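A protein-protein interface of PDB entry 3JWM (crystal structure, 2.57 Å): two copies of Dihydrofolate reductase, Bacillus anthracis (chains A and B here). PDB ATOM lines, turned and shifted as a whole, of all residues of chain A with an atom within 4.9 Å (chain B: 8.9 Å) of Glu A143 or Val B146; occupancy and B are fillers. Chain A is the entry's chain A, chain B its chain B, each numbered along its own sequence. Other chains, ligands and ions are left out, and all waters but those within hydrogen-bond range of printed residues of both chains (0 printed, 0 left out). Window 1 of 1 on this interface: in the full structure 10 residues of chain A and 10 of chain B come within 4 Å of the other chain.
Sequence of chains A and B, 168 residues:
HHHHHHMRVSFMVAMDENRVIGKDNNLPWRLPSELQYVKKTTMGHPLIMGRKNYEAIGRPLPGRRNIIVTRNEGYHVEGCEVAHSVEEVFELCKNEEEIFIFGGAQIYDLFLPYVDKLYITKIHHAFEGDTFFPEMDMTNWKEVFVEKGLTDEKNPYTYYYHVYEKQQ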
ATOM      1  N   TRP A 141      13.809   1.810 -34.465  1.00  0.00           N
ATOM      2  CA  TRP A 141      13.405   3.199 -34.293  1.00  0.00           C
ATOM      3  C   TRP A 141      12.495   3.335 -33.090  1.00  0.00           C
ATOM      4  O   TRP A 141      11.697   2.448 -32.807  1.00  0.00           O
ATOM      5  CB  TRP A 141      12.709   3.723 -35.537  1.00  0.00           C
ATOM      6  CG  TRP A 141      13.615   3.926 -36.704  1.00  0.00           C
ATOM      7  CD1 TRP A 141      14.213   2.956 -37.463  1.00  0.00           C
ATOM      8  CD2 TRP A 141      14.009   5.178 -37.267  1.00  0.00           C
ATOM      9  NE1 TRP A 141      14.959   3.530 -38.459  1.00  0.00           N
ATOM     10  CE2 TRP A 141      14.851   4.893 -38.366  1.00  0.00           C
ATOM     11  CE3 TRP A 141      13.726   6.516 -36.957  1.00  0.00           C
ATOM     12  CZ2 TRP A 141      15.418   5.892 -39.151  1.00  0.00           C
ATOM     13  CZ3 TRP A 141      14.292   7.510 -37.737  1.00  0.00           C
ATOM     14  CH2 TRP A 141      15.130   7.190 -38.823  1.00  0.00           C
ATOM     15  N   LYS A 142      12.634   4.443 -32.375  1.00  0.00           N
ATOM     16  CA  LYS A 142      11.803   4.717 -31.207  1.00  0.00           C
ATOM     17  C   LYS A 142      11.155   6.078 -31.341  1.00  0.00           C
ATOM     18  O   LYS A 142      11.809   7.050 -31.733  1.00  0.00           O
ATOM     19  CB  LYS A 142      12.621   4.670 -29.922  1.00  0.00           C
ATOM     20  CG  LYS A 142      12.909   3.279 -29.428  1.00  0.00           C
ATOM     21  CD  LYS A 142      13.685   3.326 -28.126  1.00  0.00           C
ATOM     22  CE  LYS A 142      14.118   1.937 -27.703  1.00  0.00           C
ATOM     23  NZ  LYS A 142      15.021   2.017 -26.534  1.00  0.00           N
ATOM     24  N   GLU A 143       9.865   6.141 -31.029  1.00  0.00           N
ATOM     25  CA  GLU A 143       9.158   7.409 -30.980  1.00  0.00           C
ATOM     26  C   GLU A 143       9.630   8.157 -29.741  1.00  0.00           C
ATOM     27  O   GLU A 143       9.615   7.615 -28.631  1.00  0.00           O
ATOM     28  CB  GLU A 143       7.646   7.189 -30.924  1.00  0.00           C
ATOM     29  CG  GLU A 143       6.816   8.402 -31.324  1.00  0.00           C
ATOM     30  CD  GLU A 143       5.324   8.146 -31.235  1.00  0.00           C
ATOM     31  OE1 GLU A 143       4.665   8.120 -32.290  1.00  0.00           O
ATOM     32  OE2 GLU A 143       4.812   7.956 -30.114  1.00  0.00           O
ATOM     33  N   VAL A 144      10.072   9.394 -29.931  1.00  0.00           N
ATOM     34  CA  VAL A 144      10.587  10.187 -28.814  1.00  0.00           C
ATOM     35  C   VAL A 144       9.761  11.450 -28.575  1.00  0.00           C
ATOM     36  O   VAL A 144       9.999  12.183 -27.611  1.00  0.00           O
ATOM     37  CB  VAL A 144      12.104  10.521 -28.952  1.00  0.00           C
ATOM     38  CG1 VAL A 144      12.932   9.245 -29.031  1.00  0.00           C
ATOM     39  CG2 VAL A 144      12.368  11.417 -30.157  1.00  0.00           C
ATOM     40  N   PHE A 145       8.792  11.700 -29.453  1.00  0.00           N
ATOM     41  CA  PHE A 145       7.880  12.837 -29.300  1.00  0.00           C
ATOM     42  C   PHE A 145       6.583  12.619 -30.070  1.00  0.00           C
ATOM     43  O   PHE A 145       6.596  12.194 -31.223  1.00  0.00           O
ATOM     44  CB  PHE A 145       8.542  14.150 -29.754  1.00  0.00           C
ATOM     45  CG  PHE A 145       7.692  15.372 -29.522  1.00  0.00           C
ATOM     46  CD1 PHE A 145       7.654  15.985 -28.266  1.00  0.00           C
ATOM     47  CD2 PHE A 145       6.920  15.909 -30.555  1.00  0.00           C
ATOM     48  CE1 PHE A 145       6.864  17.103 -28.038  1.00  0.00           C
ATOM     49  CE2 PHE A 145       6.122  17.039 -30.338  1.00  0.00           C
ATOM     50  CZ  PHE A 145       6.100  17.634 -29.075  1.00  0.00           C
ATOM     51  N   VAL A 146       5.470  12.932 -29.421  1.00  0.00           N
ATOM     52  CA  VAL A 146       4.155  12.914 -30.057  1.00  0.00           C
ATOM     53  C   VAL A 146       3.221  13.944 -29.393  1.00  0.00           C
ATOM     54  O   VAL A 146       3.151  14.031 -28.165  1.00  0.00           O
ATOM     55  CB  VAL A 146       3.534  11.476 -30.074  1.00  0.00           C
ATOM     56  CG1 VAL A 146       3.284  10.952 -28.641  1.00  0.00           C
ATOM     57  CG2 VAL A 146       2.263  11.422 -30.950  1.00  0.00           C
ATOM     58  N   HIS A 162       4.769  13.681 -34.943  1.00  0.00           N
ATOM     59  CA  HIS A 162       5.547  12.540 -34.451  1.00  0.00           C
ATOM     60  C   HIS A 162       7.034  12.747 -34.712  1.00  0.00           C
ATOM     61  O   HIS A 162       7.426  13.295 -35.750  1.00  0.00           O
ATOM     62  CB  HIS A 162       5.144  11.250 -35.168  1.00  0.00           C
ATOM     63  CG  HIS A 162       3.729  10.828 -34.936  1.00  0.00           C
ATOM     64  ND1 HIS A 162       3.388   9.842 -34.038  1.00  0.00           N
ATOM     65  CD2 HIS A 162       2.572  11.235 -35.510  1.00  0.00           C
ATOM     66  CE1 HIS A 162       2.077   9.672 -34.051  1.00  0.00           C
ATOM     67  NE2 HIS A 162       1.559  10.502 -34.941  1.00  0.00           N
ATOM     68  N   VAL A 163       7.862  12.284 -33.782  1.00  0.00           N
ATOM     69  CA  VAL A 163       9.310  12.255 -33.989  1.00  0.00           C
ATOM     70  C   VAL A 163       9.852  10.867 -33.637  1.00  0.00           C
ATOM     71  O   VAL A 163       9.599  10.352 -32.546  1.00  0.00           O
ATOM     72  CB  VAL A 163      10.054  13.386 -33.202  1.00  0.00           C
ATOM     73  CG1 VAL A 163      11.573  13.277 -33.361  1.00  0.00           C
ATOM     74  CG2 VAL A 163       9.594  14.768 -33.663  1.00  0.00           C
ATOM     75  N   TYR A 164      10.581  10.269 -34.578  1.00  0.00           N
ATOM     76  CA  TYR A 164      11.233   8.986 -34.367  1.00  0.00           C
ATOM     77  C   TYR A 164      12.745   9.108 -34.498  1.00  0.00           C
ATOM     78  O   TYR A 164      13.239   9.827 -35.364  1.00  0.00           O
ATOM     79  CB  TYR A 164      10.734   7.959 -35.377  1.00  0.00           C
ATOM     80  CG  TYR A 164       9.246   7.725 -35.361  1.00  0.00           C
ATOM     81  CD1 TYR A 164       8.685   6.705 -34.590  1.00  0.00           C
ATOM     82  CD2 TYR A 164       8.397   8.505 -36.140  1.00  0.00           C
ATOM     83  CE1 TYR A 164       7.307   6.483 -34.588  1.00  0.00           C
ATOM     84  CE2 TYR A 164       7.032   8.292 -36.144  1.00  0.00           C
ATOM     85  CZ  TYR A 164       6.490   7.287 -35.369  1.00  0.00           C
ATOM     86  OH  TYR A 164       5.131   7.100 -35.394  1.00  0.00           O
ATOM     87  N   TYR B  37      -3.798  -1.808 -36.248  1.00  0.00           N
ATOM     88  CA  TYR B  37      -2.353  -2.073 -36.152  1.00  0.00           C
ATOM     89  C   TYR B  37      -2.032  -3.569 -36.218  1.00  0.00           C
ATOM     90  O   TYR B  37      -1.062  -3.964 -36.851  1.00  0.00           O
ATOM     91  CB  TYR B  37      -1.776  -1.461 -34.875  1.00  0.00           C
ATOM     92  CG  TYR B  37      -0.438  -2.035 -34.452  1.00  0.00           C
ATOM     93  CD1 TYR B  37       0.759  -1.468 -34.899  1.00  0.00           C
ATOM     94  CD2 TYR B  37      -0.368  -3.151 -33.601  1.00  0.00           C
ATOM     95  CE1 TYR B  37       1.988  -1.991 -34.509  1.00  0.00           C
ATOM     96  CE2 TYR B  37       0.854  -3.682 -33.209  1.00  0.00           C
ATOM     97  CZ  TYR B  37       2.026  -3.096 -33.666  1.00  0.00           C
ATOM     98  OH  TYR B  37       3.240  -3.615 -33.275  1.00  0.00           O
ATOM     99  N   ILE B 120       3.901  -6.477 -28.494  1.00  0.00           N
ATOM    100  CA  ILE B 120       3.081  -6.376 -27.305  1.00  0.00           C
ATOM    101  C   ILE B 120       2.478  -4.961 -27.158  1.00  0.00           C
ATOM    102  O   ILE B 120       3.202  -3.958 -27.149  1.00  0.00           O
ATOM    103  CB  ILE B 120       3.913  -6.862 -26.061  1.00  0.00           C
ATOM    104  CG1 ILE B 120       3.035  -7.226 -24.853  1.00  0.00           C
ATOM    105  CG2 ILE B 120       5.046  -5.893 -25.711  1.00  0.00           C
ATOM    106  CD1 ILE B 120       2.541  -6.067 -24.045  1.00  0.00           C
ATOM    107  N   LYS B 122       0.700  -2.450 -24.674  1.00  0.00           N
ATOM    108  CA  LYS B 122       0.539  -2.228 -23.239  1.00  0.00           C
ATOM    109  C   LYS B 122      -0.507  -1.159 -22.985  1.00  0.00           C
ATOM    110  O   LYS B 122      -0.352  -0.014 -23.408  1.00  0.00           O
ATOM    111  CB  LYS B 122       1.869  -1.843 -22.583  1.00  0.00           C
ATOM    112  CG  LYS B 122       2.910  -2.950 -22.620  1.00  0.00           C
ATOM    113  CD  LYS B 122       4.171  -2.568 -21.876  1.00  0.00           C
ATOM    114  CE  LYS B 122       5.211  -3.682 -21.927  1.00  0.00           C
ATOM    115  NZ  LYS B 122       6.339  -3.390 -20.986  1.00  0.00           N
ATOM    116  N   HIS B 124      -2.648   1.174 -20.448  1.00  0.00           N
ATOM    117  CA  HIS B 124      -2.400   1.818 -19.159  1.00  0.00           C
ATOM    118  C   HIS B 124      -3.714   1.970 -18.416  1.00  0.00           C
ATOM    119  O   HIS B 124      -4.232   3.078 -18.241  1.00  0.00           O
ATOM    120  CB  HIS B 124      -1.714   3.175 -19.367  1.00  0.00           C
ATOM    121  CG  HIS B 124      -0.329   3.077 -19.937  1.00  0.00           C
ATOM    122  ND1 HIS B 124       0.605   4.079 -19.790  1.00  0.00           N
ATOM    123  CD2 HIS B 124       0.286   2.094 -20.641  1.00  0.00           C
ATOM    124  CE1 HIS B 124       1.731   3.722 -20.384  1.00  0.00           C
ATOM    125  NE2 HIS B 124       1.564   2.521 -20.908  1.00  0.00           N
ATOM    126  N   GLU B 143      14.314  -3.961 -26.724  1.00  0.00           N
ATOM    127  CA  GLU B 143      13.207  -3.214 -27.313  1.00  0.00           C
ATOM    128  C   GLU B 143      13.685  -2.577 -28.615  1.00  0.00           C
ATOM    129  O   GLU B 143      14.667  -1.830 -28.625  1.00  0.00           O
ATOM    130  CB  GLU B 143      12.678  -2.147 -26.356  1.00  0.00           C
ATOM    131  CG  GLU B 143      11.330  -1.571 -26.775  1.00  0.00           C
ATOM    132  CD  GLU B 143      10.954  -0.314 -26.023  1.00  0.00           C
ATOM    133  OE1 GLU B 143       9.757  -0.153 -25.705  1.00  0.00           O
ATOM    134  OE2 GLU B 143      11.839   0.524 -25.748  1.00  0.00           O
ATOM    135  N   VAL B 144      13.000  -2.887 -29.709  1.00  0.00           N
ATOM    136  CA  VAL B 144      13.404  -2.398 -31.026  1.00  0.00           C
ATOM    137  C   VAL B 144      12.412  -1.389 -31.615  1.00  0.00           C
ATOM    138  O   VAL B 144      12.674  -0.805 -32.667  1.00  0.00           O
ATOM    139  CB  VAL B 144      13.629  -3.566 -32.020  1.00  0.00           C
ATOM    140  CG1 VAL B 144      14.823  -4.427 -31.590  1.00  0.00           C
ATOM    141  CG2 VAL B 144      12.350  -4.410 -32.191  1.00  0.00           C
ATOM    142  N   PHE B 145      11.281  -1.195 -30.933  1.00  0.00           N
ATOM    143  CA  PHE B 145      10.258  -0.263 -31.377  1.00  0.00           C
ATOM    144  C   PHE B 145       9.260   0.052 -30.268  1.00  0.00           C
ATOM    145  O   PHE B 145       8.798  -0.844 -29.550  1.00  0.00           O
ATOM    146  CB  PHE B 145       9.526  -0.793 -32.627  1.00  0.00           C
ATOM    147  CG  PHE B 145       8.513   0.169 -33.191  1.00  0.00           C
ATOM    148  CD1 PHE B 145       8.922   1.286 -33.915  1.00  0.00           C
ATOM    149  CD2 PHE B 145       7.155  -0.034 -32.983  1.00  0.00           C
ATOM    150  CE1 PHE B 145       7.992   2.190 -34.426  1.00  0.00           C
ATOM    151  CE2 PHE B 145       6.209   0.862 -33.491  1.00  0.00           C
ATOM    152  CZ  PHE B 145       6.632   1.978 -34.217  1.00  0.00           C
ATOM    153  N   VAL B 146       8.939   1.337 -30.137  1.00  0.00           N
ATOM    154  CA  VAL B 146       7.886   1.809 -29.236  1.00  0.00           C
ATOM    155  C   VAL B 146       7.213   3.058 -29.828  1.00  0.00           C
ATOM    156  O   VAL B 146       7.883   3.950 -30.349  1.00  0.00           O
ATOM    157  CB  VAL B 146       8.419   2.087 -27.791  1.00  0.00           C
ATOM    158  CG1 VAL B 146       9.455   3.224 -27.764  1.00  0.00           C
ATOM    159  CG2 VAL B 146       7.270   2.396 -26.835  1.00  0.00           C
ATOM    160  N   GLU B 147       5.888   3.103 -29.768  1.00  0.00           N
ATOM    161  CA  GLU B 147       5.145   4.315 -30.122  1.00  0.00           C
ATOM    162  C   GLU B 147       3.794   4.335 -29.429  1.00  0.00           C
ATOM    163  O   GLU B 147       3.225   3.285 -29.126  1.00  0.00           O
ATOM    164  CB  GLU B 147       5.004   4.503 -31.647  1.00  0.00           C
ATOM    165  CG  GLU B 147       3.956   3.628 -32.324  1.00  0.00           C
ATOM    166  CD  GLU B 147       3.630   4.060 -33.744  1.00  0.00           C
ATOM    167  OE1 GLU B 147       4.503   4.639 -34.424  1.00  0.00           O
ATOM    168  OE2 GLU B 147       2.489   3.811 -34.194  1.00  0.00           O
ATOM    169  N   LYS B 148       3.306   5.547 -29.167  1.00  0.00           N
ATOM    170  CA  LYS B 148       2.030   5.749 -28.516  1.00  0.00           C
ATOM    171  C   LYS B 148       0.911   5.355 -29.470  1.00  0.00           C
ATOM    172  O   LYS B 148       0.955   5.681 -30.648  1.00  0.00           O
ATOM    173  CB  LYS B 148       1.890   7.209 -28.092  1.00  0.00           C
ATOM    174  CG  LYS B 148       0.765   7.483 -27.101  1.00  0.00           C
ATOM    175  CD  LYS B 148       0.706   8.955 -26.729  1.00  0.00           C
ATOM    176  CE  LYS B 148      -0.103   9.190 -25.459  1.00  0.00           C
ATOM    177  NZ  LYS B 148      -1.523   8.757 -25.552  1.00  0.00           N
ATOM    178  N   GLY B 149      -0.076   4.629 -28.959  1.00  0.00           N
ATOM    179  CA  GLY B 149      -1.270   4.326 -29.728  1.00  0.00           C
ATOM    180  C   GLY B 149      -2.189   5.529 -29.786  1.00  0.00           C
ATOM    181  O   GLY B 149      -2.015   6.497 -29.035  1.00  0.00           O
ATOM    182  N   LEU B 150      -3.175   5.464 -30.675  1.00  0.00           N
ATOM    183  CA  LEU B 150      -4.132   6.549 -30.856  1.00  0.00           C
ATOM    184  C   LEU B 150      -5.185   6.527 -29.746  1.00  0.00           C
ATOM    185  O   LEU B 150      -5.957   5.574 -29.634  1.00  0.00           O
ATOM    186  CB  LEU B 150      -4.815   6.425 -32.222  1.00  0.00           C
ATOM    187  CG  LEU B 150      -5.407   7.640 -32.954  1.00  0.00           C
ATOM    188  CD1 LEU B 150      -6.759   7.256 -33.532  1.00  0.00           C
ATOM    189  CD2 LEU B 150      -5.523   8.932 -32.113  1.00  0.00           C
ATOM    190  N   TYR B 159      -2.410   3.696 -24.435  1.00  0.00           N
ATOM    191  CA  TYR B 159      -1.713   2.443 -24.737  1.00  0.00           C
ATOM    192  C   TYR B 159      -0.512   2.657 -25.656  1.00  0.00           C
ATOM    193  O   TYR B 159      -0.475   3.617 -26.437  1.00  0.00           O
ATOM    194  CB  TYR B 159      -2.680   1.407 -25.343  1.00  0.00           C
ATOM    195  CG  TYR B 159      -3.361   1.833 -26.633  1.00  0.00           C
ATOM    196  CD1 TYR B 159      -2.983   1.282 -27.851  1.00  0.00           C
ATOM    197  CD2 TYR B 159      -4.396   2.781 -26.629  1.00  0.00           C
ATOM    198  CE1 TYR B 159      -3.607   1.656 -29.039  1.00  0.00           C
ATOM    199  CE2 TYR B 159      -5.025   3.166 -27.814  1.00  0.00           C
ATOM    200  CZ  TYR B 159      -4.623   2.597 -29.014  1.00  0.00           C
ATOM    201  OH  TYR B 159      -5.232   2.966 -30.191  1.00  0.00           O
ATOM    202  N   TYR B 160       0.464   1.758 -25.561  1.00  0.00           N
ATOM    203  CA  TYR B 160       1.697   1.869 -26.350  1.00  0.00           C
ATOM    204  C   TYR B 160       1.981   0.567 -27.074  1.00  0.00           C
ATOM    205  O   TYR B 160       1.777  -0.505 -26.516  1.00  0.00           O
ATOM    206  CB  TYR B 160       2.889   2.251 -25.455  1.00  0.00           C
ATOM    207  CG  TYR B 160       2.871   3.692 -24.997  1.00  0.00           C
ATOM    208  CD1 TYR B 160       2.027   4.106 -23.966  1.00  0.00           C
ATOM    209  CD2 TYR B 160       3.696   4.646 -25.591  1.00  0.00           C
ATOM    210  CE1 TYR B 160       2.000   5.424 -23.547  1.00  0.00           C
ATOM    211  CE2 TYR B 160       3.675   5.973 -25.176  1.00  0.00           C
ATOM    212  CZ  TYR B 160       2.820   6.353 -24.157  1.00  0.00           C
ATOM    213  OH  TYR B 160       2.776   7.663 -23.735  1.00  0.00           O
ATOM    214  N   TYR B 161       2.426   0.666 -28.324  1.00  0.00           N
ATOM    215  CA  TYR B 161       2.909  -0.489 -29.072  1.00  0.00           C
ATOM    216  C   TYR B 161       4.376  -0.707 -28.731  1.00  0.00           C
ATOM    217  O   TYR B 161       5.171   0.219 -28.824  1.00  0.00           O
ATOM    218  CB  TYR B 161       2.767  -0.274 -30.585  1.00  0.00           C
ATOM    219  CG  TYR B 161       1.360   0.024 -31.062  1.00  0.00           C
ATOM    220  CD1 TYR B 161       1.042   1.262 -31.641  1.00  0.00           C
ATOM    221  CD2 TYR B 161       0.339  -0.926 -30.928  1.00  0.00           C
ATOM    222  CE1 TYR B 161      -0.258   1.544 -32.080  1.00  0.00           C
ATOM    223  CE2 TYR B 161      -0.962  -0.653 -31.357  1.00  0.00           C
ATOM    224  CZ  TYR B 161      -1.253   0.580 -31.934  1.00  0.00           C
ATOM    225  OH  TYR B 161      -2.542   0.833 -32.362  1.00  0.00           O
ATOM    226  N   HIS B 162       4.724  -1.922 -28.311  1.00  0.00           N
ATOM    227  CA  HIS B 162       6.110  -2.279 -28.022  1.00  0.00           C
ATOM    228  C   HIS B 162       6.516  -3.493 -28.839  1.00  0.00           C
ATOM    229  O   HIS B 162       5.717  -4.408 -29.040  1.00  0.00           O
ATOM    230  CB  HIS B 162       6.302  -2.627 -26.553  1.00  0.00           C
ATOM    231  CG  HIS B 162       6.105  -1.485 -25.601  1.00  0.00           C
ATOM    232  ND1 HIS B 162       7.153  -0.734 -25.111  1.00  0.00           N
ATOM    233  CD2 HIS B 162       4.991  -1.020 -24.985  1.00  0.00           C
ATOM    234  CE1 HIS B 162       6.688   0.166 -24.263  1.00  0.00           C
ATOM    235  NE2 HIS B 162       5.379   0.012 -24.166  1.00  0.00           N
ATOM    236  N   VAL B 163       7.755  -3.496 -29.320  1.00  0.00           N
ATOM    237  CA  VAL B 163       8.313  -4.672 -29.980  1.00  0.00           C
ATOM    238  C   VAL B 163       9.673  -5.025 -29.360  1.00  0.00           C
ATOM    239  O   VAL B 163      10.535  -4.163 -29.189  1.00  0.00           O
ATOM    240  CB  VAL B 163       8.398  -4.515 -31.526  1.00  0.00           C
ATOM    241  CG1 VAL B 163       8.813  -5.815 -32.167  1.00  0.00           C
ATOM    242  CG2 VAL B 163       7.048  -4.079 -32.112  1.00  0.00           C
ATOM    243  N   TYR B 164       9.835  -6.296 -28.997  1.00  0.00           N
ATOM    244  CA  TYR B 164      11.089  -6.790 -28.433  1.00  0.00           C
ATOM    245  C   TYR B 164      11.621  -7.937 -29.278  1.00  0.00           C
ATOM    246  O   TYR B 164      10.853  -8.763 -29.780  1.00  0.00           O
ATOM    247  CB  TYR B 164      10.909  -7.270 -26.988  1.00  0.00           C
ATOM    248  CG  TYR B 164      10.313  -6.260 -26.028  1.00  0.00           C
ATOM    249  CD1 TYR B 164      11.133  -5.453 -25.227  1.00  0.00           C
ATOM    250  CD2 TYR B 164       8.926  -6.130 -25.902  1.00  0.00           C
ATOM    251  CE1 TYR B 164      10.579  -4.526 -24.332  1.00  0.00           C
ATOM    252  CE2 TYR B 164       8.364  -5.210 -25.024  1.00  0.00           C
ATOM    253  CZ  TYR B 164       9.190  -4.415 -24.235  1.00  0.00           C
ATOM    254  OH  TYR B 164       8.610  -3.514 -23.364  1.00  0.00           O
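The backbone NH of Trp A141 sits at hydrogen-bond distance from the backbone carbonyl oxygen of Val B144.
NZ of Lys A142 lies within salt-bridge range of OE2 of Glu B143 (3.6 Å).
O of Val B146 is in hydrogen-bond range of N of Glu A143 (3.0 Å).
OE2 of Glu A143 is in hydrogen-bond range of N of Lys B148.
The side-chain carboxylate of Glu B147 is in hydrogen-bond range of the side-chain hydroxyl of Tyr A164, 2.7 Å away.
The side-chain carboxylate of Glu A143 lies within hydrogen-bond range of a ring nitrogen (ND1) of His A162 (2.8 Å).
The side-chain hydroxyl (OH) of Tyr A164 sits at hydrogen-bond distance from the side-chain carboxylate (OE1) of Glu A143, at 3.3 Å.
The side-chain carboxylate (OE1) of Glu B143 sits at hydrogen-bond distance from a ring nitrogen (ND1) of His B162 (2.7 Å).
The backbone NH (N) of Val B144 lies within hydrogen-bond range of the backbone carbonyl oxygen (O) of Val B163, 2.8 Å away.
The backbone NH (N) of Val B163 lies within hydrogen-bond range of the backbone carbonyl oxygen (O) of Phe B145 (2.9 Å).
The backbone carbonyl oxygen of Glu B147 sits at hydrogen-bond distance from the backbone NH of Tyr B161, 2.9 Å away.
O of Trp A141 touches CD1 of Phe B145 (3.2 Å).
O of Trp A141 touches N of Val B146, 3.996 Å away.
Lys A142 touches Val B146.
OE2 of Glu A143 touches CA of Glu B147, 3.7 Å away.
Val A146 touches Lys B148.
Printed residues of chain B within 4 Å of Glu A143: Val B146 (3.0 Å), Glu B147 (3.7 Å) and Lys B148 (3.0 Å).
Val A144 touches none of the printed residues of chain B.
Printed residues of chain B within 4 Å of Val A146: Lys B148.
Of the printed residues of chain A, Glu B143 touches Lys A142.
Of the printed residues of chain A, Val B146 touches Trp A141 (3.996 Å), Lys A142 (3.8 Å) and Glu A143 (3.0 Å).
Printed residues of chain A within 4 Å of Glu B147: Glu A143 and Tyr A164.
Printed residues of chain A within 4 Å of Lys B148: Glu A143 and Val A146.
The nearest residue of chain B that does not touch Glu A143 is Tyr B160 (5.4 Å).
The nearest printed residue of chain B that does not touch Tyr A164 is Phe B145 (4.4 Å).
Of the 9 printed residues of chain A, 5 touch a printed residue of chain B.
Hydrophobic or aromatic side chains of chain B that line the printed part of chain A: Phe B145 and Val B146.
Glu A143 touches Val B146, but with the chains exchanged Val A146 does not touch Glu B143 (13.2 Å).
Positions printed for both chains: 143, 144, 145, 146, 162, 163 and 164.
Of the 10 pairs that touch across the chains among the printed residues, none has its exchanged pair printed and touching as well.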
